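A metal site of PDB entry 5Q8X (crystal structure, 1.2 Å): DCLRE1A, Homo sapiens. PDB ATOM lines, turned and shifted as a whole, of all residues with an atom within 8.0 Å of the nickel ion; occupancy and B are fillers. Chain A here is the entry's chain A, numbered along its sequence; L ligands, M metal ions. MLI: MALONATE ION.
ND1 of His 96 is in hydrogen-bond range of O of Glu 296, at 2.7 Å.
The side-chain hydroxyl (OG1) of Thr 34 lies within hydrogen-bond range of a ring nitrogen (ND1) of His 35 (2.9 Å).
A ring nitrogen (NE2) of His 37 sits at hydrogen-bond distance from the backbone carbonyl oxygen (O) of Ile 184 (2.9 Å).
NE2 of His 40 sits close to OD2 of Asp 118 (3.3 Å).
The nickel ion is bound by O8 of the ligand (2.0 Å), OD2 of Asp 118 (2.2 Å), O7 of the ligand (2.2 Å), NE2 of His 35 (2.2 Å), ND1 of His 37 (2.2 Å) and NE2 of His 96 (2.3 Å).
Four residues have an atom within 4 Å of the nickel ion: His 35, His 37, His 96 and Asp 118.
Along chain A the residues within 4 Å of the nickel ion span positions 35 to 118.
The nearest printed residue that does not touch the nickel ion is His 40 (4.2 Å).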
ATOM      1  N   ASP A  18     -24.753  -1.779   1.918  1.00  0.00           N
ATOM      2  CA  ASP A  18     -25.266  -1.228   3.226  1.00  0.00           C
ATOM      3  C   ASP A  18     -26.479  -2.069   3.769  1.00  0.00           C
ATOM      4  O   ASP A  18     -27.479  -1.488   4.273  1.00  0.00           O
ATOM      5  CB  ASP A  18     -25.516   0.249   3.122  1.00  0.00           C
ATOM      6  CG  ASP A  18     -24.226   1.063   2.738  1.00  0.00           C
ATOM      7  OD1 ASP A  18     -23.137   0.494   2.824  1.00  0.00           O
ATOM      8  OD2 ASP A  18     -24.448   2.301   2.395  1.00  0.00           O
ATOM      9  N   THR A  34     -20.440   1.263   2.313  1.00  0.00           N
ATOM     10  CA  THR A  34     -20.017   2.536   1.708  1.00  0.00           C
ATOM     11  C   THR A  34     -19.248   3.399   2.726  1.00  0.00           C
ATOM     12  O   THR A  34     -18.311   4.128   2.332  1.00  0.00           O
ATOM     13  CB  THR A  34     -21.133   3.355   1.070  1.00  0.00           C
ATOM     14  OG1 THR A  34     -22.112   3.718   2.101  1.00  0.00           O
ATOM     15  CG2 THR A  34     -21.823   2.600  -0.046  1.00  0.00           C
ATOM     16  N   HIS A  35     -19.655   3.370   4.007  1.00  0.00           N
ATOM     17  CA  HIS A  35     -19.045   4.230   5.057  1.00  0.00           C
ATOM     18  C   HIS A  35     -19.461   3.772   6.420  1.00  0.00           C
ATOM     19  O   HIS A  35     -20.533   3.129   6.592  1.00  0.00           O
ATOM     20  CB  HIS A  35     -19.371   5.740   4.780  1.00  0.00           C
ATOM     21  CG  HIS A  35     -20.788   6.171   4.936  1.00  0.00           C
ATOM     22  ND1 HIS A  35     -21.850   5.801   4.121  1.00  0.00           N
ATOM     23  CD2 HIS A  35     -21.322   7.010   5.845  1.00  0.00           C
ATOM     24  CE1 HIS A  35     -22.957   6.444   4.550  1.00  0.00           C
ATOM     25  NE2 HIS A  35     -22.633   7.193   5.559  1.00  0.00           N
ATOM     26  N   PHE A  36     -18.694   4.222   7.396  1.00  0.00           N
ATOM     27  CA  PHE A  36     -18.947   3.890   8.820  1.00  0.00           C
ATOM     28  C   PHE A  36     -19.883   4.850   9.538  1.00  0.00           C
ATOM     29  O   PHE A  36     -19.467   5.590  10.487  1.00  0.00           O
ATOM     30  CB  PHE A  36     -17.577   3.771   9.561  1.00  0.00           C
ATOM     31  CG  PHE A  36     -17.630   3.061  10.899  1.00  0.00           C
ATOM     32  CD1 PHE A  36     -17.701   1.663  10.932  1.00  0.00           C
ATOM     33  CD2 PHE A  36     -17.559   3.765  12.107  1.00  0.00           C
ATOM     34  CE1 PHE A  36     -17.731   0.995  12.183  1.00  0.00           C
ATOM     35  CE2 PHE A  36     -17.567   3.107  13.340  1.00  0.00           C
ATOM     36  CZ  PHE A  36     -17.654   1.760  13.381  1.00  0.00           C
ATOM     37  N   HIS A  37     -21.174   4.880   9.156  1.00  0.00           N
ATOM     38  CA  HIS A  37     -22.296   5.530   9.870  1.00  0.00           C
ATOM     39  C   HIS A  37     -23.304   4.438  10.249  1.00  0.00           C
ATOM     40  O   HIS A  37     -23.578   3.513   9.475  1.00  0.00           O
ATOM     41  CB  HIS A  37     -22.988   6.660   9.061  1.00  0.00           C
ATOM     42  CG  HIS A  37     -22.235   7.971   9.049  1.00  0.00           C
ATOM     43  ND1 HIS A  37     -22.463   8.984   8.107  1.00  0.00           N
ATOM     44  CD2 HIS A  37     -21.291   8.452   9.891  1.00  0.00           C
ATOM     45  CE1 HIS A  37     -21.744  10.044   8.404  1.00  0.00           C
ATOM     46  NE2 HIS A  37     -20.999   9.728   9.448  1.00  0.00           N
ATOM     47  N   SER A  38     -23.885   4.575  11.459  1.00  0.00           N
ATOM     48  CA  SER A  38     -24.657   3.476  12.116  1.00  0.00           C
ATOM     49  C   SER A  38     -25.845   3.071  11.289  1.00  0.00           C
ATOM     50  O   SER A  38     -26.077   1.833  11.266  1.00  0.00           O
ATOM     51  CB  SER A  38     -24.928   3.800  13.605  1.00  0.00           C
ATOM     52  OG  SER A  38     -25.712   4.934  13.703  1.00  0.00           O
ATOM     53  N   ASP A  39     -26.592   3.957  10.655  1.00  0.00           N
ATOM     54  CA  ASP A  39     -27.780   3.519   9.827  1.00  0.00           C
ATOM     55  C   ASP A  39     -27.313   2.586   8.685  1.00  0.00           C
ATOM     56  O   ASP A  39     -28.112   1.761   8.163  1.00  0.00           O
ATOM     57  CB  ASP A  39     -28.523   4.680   9.248  1.00  0.00           C
ATOM     58  CG  ASP A  39     -29.512   5.390  10.249  1.00  0.00           C
ATOM     59  OD1 ASP A  39     -29.615   4.942  11.402  1.00  0.00           O
ATOM     60  OD2 ASP A  39     -30.097   6.408   9.805  1.00  0.00           O
ATOM     61  N   HIS A  40     -26.035   2.707   8.263  1.00  0.00           N
ATOM     62  CA  HIS A  40     -25.487   1.878   7.148  1.00  0.00           C
ATOM     63  C   HIS A  40     -24.799   0.636   7.588  1.00  0.00           C
ATOM     64  O   HIS A  40     -24.981  -0.406   6.908  1.00  0.00           O
ATOM     65  CB  HIS A  40     -24.527   2.807   6.292  1.00  0.00           C
ATOM     66  CG  HIS A  40     -25.241   3.956   5.694  1.00  0.00           C
ATOM     67  ND1 HIS A  40     -25.653   4.010   4.365  1.00  0.00           N
ATOM     68  CD2 HIS A  40     -25.664   5.126   6.230  1.00  0.00           C
ATOM     69  CE1 HIS A  40     -26.284   5.127   4.146  1.00  0.00           C
ATOM     70  NE2 HIS A  40     -26.340   5.814   5.278  1.00  0.00           N
ATOM     71  N   HIS A  96     -17.938  12.738   1.706  1.00  0.00           N
ATOM     72  CA  HIS A  96     -18.876  12.588   2.839  1.00  0.00           C
ATOM     73  C   HIS A  96     -17.999  12.616   4.063  1.00  0.00           C
ATOM     74  O   HIS A  96     -17.374  13.691   4.295  1.00  0.00           O
ATOM     75  CB  HIS A  96     -19.816  11.387   2.643  1.00  0.00           C
ATOM     76  CG  HIS A  96     -20.883  11.145   3.672  1.00  0.00           C
ATOM     77  ND1 HIS A  96     -21.761  12.130   4.020  1.00  0.00           N
ATOM     78  CD2 HIS A  96     -21.172  10.069   4.464  1.00  0.00           C
ATOM     79  CE1 HIS A  96     -22.595  11.647   4.962  1.00  0.00           C
ATOM     80  NE2 HIS A  96     -22.300  10.374   5.224  1.00  0.00           N
ATOM     81  N   CYS A  97     -17.972  11.591   4.885  1.00  0.00           N
ATOM     82  CA  CYS A  97     -17.068  11.479   6.082  1.00  0.00           C
ATOM     83  C   CYS A  97     -15.777  10.700   5.683  1.00  0.00           C
ATOM     84  O   CYS A  97     -15.693  10.119   4.613  1.00  0.00           O
ATOM     85  CB  CYS A  97     -17.854  10.783   7.217  1.00  0.00           C
ATOM     86  SG  CYS A  97     -18.315   9.013   6.813  1.00  0.00           S
ATOM     87  N   ALA A 100     -15.546   7.306   3.318  1.00  0.00           N
ATOM     88  CA  ALA A 100     -16.787   7.149   2.543  1.00  0.00           C
ATOM     89  C   ALA A 100     -16.513   7.045   1.059  1.00  0.00           C
ATOM     90  O   ALA A 100     -15.780   7.874   0.496  1.00  0.00           O
ATOM     91  CB  ALA A 100     -17.791   8.253   2.858  1.00  0.00           C
ATOM     92  N   GLY A 117     -23.552   5.848  -2.339  1.00  0.00           N
ATOM     93  CA  GLY A 117     -23.594   5.848  -0.884  1.00  0.00           C
ATOM     94  C   GLY A 117     -24.206   7.145  -0.407  1.00  0.00           C
ATOM     95  O   GLY A 117     -25.083   7.712  -1.042  1.00  0.00           O
ATOM     96  N   ASP A 118     -23.659   7.654   0.695  1.00  0.00           N
ATOM     97  CA  ASP A 118     -23.888   9.082   1.090  1.00  0.00           C
ATOM     98  C   ASP A 118     -22.800   9.942   0.441  1.00  0.00           C
ATOM     99  O   ASP A 118     -21.604   9.578   0.487  1.00  0.00           O
ATOM    100  CB  ASP A 118     -23.889   9.270   2.600  1.00  0.00           C
ATOM    101  CG  ASP A 118     -25.172   8.833   3.334  1.00  0.00           C
ATOM    102  OD1 ASP A 118     -26.202   8.520   2.684  1.00  0.00           O
ATOM    103  OD2 ASP A 118     -25.151   8.867   4.590  1.00  0.00           O
ATOM    104  N   PHE A 119     -23.182  11.085  -0.120  1.00  0.00           N
ATOM    105  CA  PHE A 119     -22.190  11.956  -0.804  1.00  0.00           C
ATOM    106  C   PHE A 119     -22.547  13.412  -0.763  1.00  0.00           C
ATOM    107  O   PHE A 119     -23.706  13.751  -0.612  1.00  0.00           O
ATOM    108  CB  PHE A 119     -21.860  11.500  -2.288  1.00  0.00           C
ATOM    109  CG  PHE A 119     -22.781  11.947  -3.443  1.00  0.00           C
ATOM    110  CD1 PHE A 119     -22.265  12.297  -4.660  1.00  0.00           C
ATOM    111  CD2 PHE A 119     -24.189  12.010  -3.307  1.00  0.00           C
ATOM    112  CE1 PHE A 119     -23.064  12.634  -5.730  1.00  0.00           C
ATOM    113  CE2 PHE A 119     -24.998  12.410  -4.371  1.00  0.00           C
ATOM    114  CZ  PHE A 119     -24.411  12.705  -5.577  1.00  0.00           C
ATOM    115  N   ASP A 141     -28.063   9.272  -3.324  1.00  0.00           N
ATOM    116  CA  ASP A 141     -28.332   9.909  -1.976  1.00  0.00           C
ATOM    117  C   ASP A 141     -29.129  11.181  -2.262  1.00  0.00           C
ATOM    118  O   ASP A 141     -28.625  12.242  -2.646  1.00  0.00           O
ATOM    119  CB  ASP A 141     -26.995  10.254  -1.281  1.00  0.00           C
ATOM    120  CG  ASP A 141     -27.139  11.178  -0.098  1.00  0.00           C
ATOM    121  OD1 ASP A 141     -28.294  11.306   0.401  1.00  0.00           O
ATOM    122  OD2 ASP A 141     -26.092  11.673   0.358  1.00  0.00           O
ATOM    123  N   THR A 143     -30.929  12.800   0.185  1.00  0.00           N
ATOM    124  CA  THR A 143     -31.228  13.415   1.480  1.00  0.00           C
ATOM    125  C   THR A 143     -31.887  14.773   1.359  1.00  0.00           C
ATOM    126  O   THR A 143     -32.979  15.034   1.984  1.00  0.00           O
ATOM    127  CB  THR A 143     -29.946  13.483   2.351  1.00  0.00           C
ATOM    128  OG1 THR A 143     -29.448  12.164   2.649  1.00  0.00           O
ATOM    129  CG2 THR A 143     -30.252  14.140   3.697  1.00  0.00           C
ATOM    130  N   SER A 183     -20.738  10.944  15.669  1.00  0.00           N
ATOM    131  CA  SER A 183     -20.351  10.018  14.617  1.00  0.00           C
ATOM    132  C   SER A 183     -19.054  10.565  14.002  1.00  0.00           C
ATOM    133  O   SER A 183     -18.650  11.717  14.299  1.00  0.00           O
ATOM    134  CB  SER A 183     -21.415   9.952  13.493  1.00  0.00           C
ATOM    135  OG  SER A 183     -21.617  11.246  12.942  1.00  0.00           O
ATOM    136  N   ILE A 184     -18.405   9.836  13.134  1.00  0.00           N
ATOM    137  CA  ILE A 184     -17.325  10.375  12.344  1.00  0.00           C
ATOM    138  C   ILE A 184     -17.914  11.333  11.327  1.00  0.00           C
ATOM    139  O   ILE A 184     -19.161  11.297  11.019  1.00  0.00           O
ATOM    140  CB  ILE A 184     -16.472   9.274  11.630  1.00  0.00           C
ATOM    141  CG1 ILE A 184     -17.225   8.496  10.575  1.00  0.00           C
ATOM    142  CG2 ILE A 184     -15.819   8.392  12.706  1.00  0.00           C
ATOM    143  CD1 ILE A 184     -16.352   7.653   9.696  1.00  0.00           C
ATOM    144  N   GLU A 296     -22.351  17.455   5.111  1.00  0.00           N
ATOM    145  CA  GLU A 296     -21.640  16.395   4.317  1.00  0.00           C
ATOM    146  C   GLU A 296     -22.560  15.658   3.290  1.00  0.00           C
ATOM    147  O   GLU A 296     -22.244  14.558   2.826  1.00  0.00           O
ATOM    148  CB  GLU A 296     -20.837  15.468   5.181  1.00  0.00           C
ATOM    149  CG  GLU A 296     -19.620  16.195   5.875  1.00  0.00           C
ATOM    150  CD  GLU A 296     -18.683  15.307   6.676  1.00  0.00           C
ATOM    151  OE1 GLU A 296     -19.072  14.196   7.134  1.00  0.00           O
ATOM    152  OE2 GLU A 296     -17.524  15.782   6.935  1.00  0.00           O
ATOM    153  N   HIS A 297     -23.731  16.287   3.021  1.00  0.00           N
ATOM    154  CA  HIS A 297     -24.590  15.851   1.909  1.00  0.00           C
ATOM    155  C   HIS A 297     -24.788  16.983   0.862  1.00  0.00           C
ATOM    156  O   HIS A 297     -24.729  18.173   1.192  1.00  0.00           O
ATOM    157  CB  HIS A 297     -26.036  15.419   2.424  1.00  0.00           C
ATOM    158  CG  HIS A 297     -26.036  14.255   3.326  1.00  0.00           C
ATOM    159  ND1 HIS A 297     -26.108  12.960   2.865  1.00  0.00           N
ATOM    160  CD2 HIS A 297     -26.110  14.159   4.700  1.00  0.00           C
ATOM    161  CE1 HIS A 297     -26.185  12.124   3.904  1.00  0.00           C
ATOM    162  NE2 HIS A 297     -26.103  12.851   4.997  1.00  0.00           N
HETATM  163  C1  MLI L   1     -25.934   9.832   8.683  1.00  0.00           C
HETATM  164  C2  MLI L   1     -25.703  10.974   7.674  1.00  0.00           C
HETATM  165  C3  MLI L   1     -26.109   8.431   8.059  1.00  0.00           C
HETATM  166  O6  MLI L   1     -26.306  12.052   7.682  1.00  0.00           O
HETATM  167  O7  MLI L   1     -24.821  10.822   6.862  1.00  0.00           O
HETATM  168  O8  MLI L   1     -25.250   8.052   7.230  1.00  0.00           O
HETATM  169  O9  MLI L   1     -27.041   7.692   8.544  1.00  0.00           O
HETATM  170 NI    NI M   1     -23.755   8.998   6.274  1.00  0.00          NI
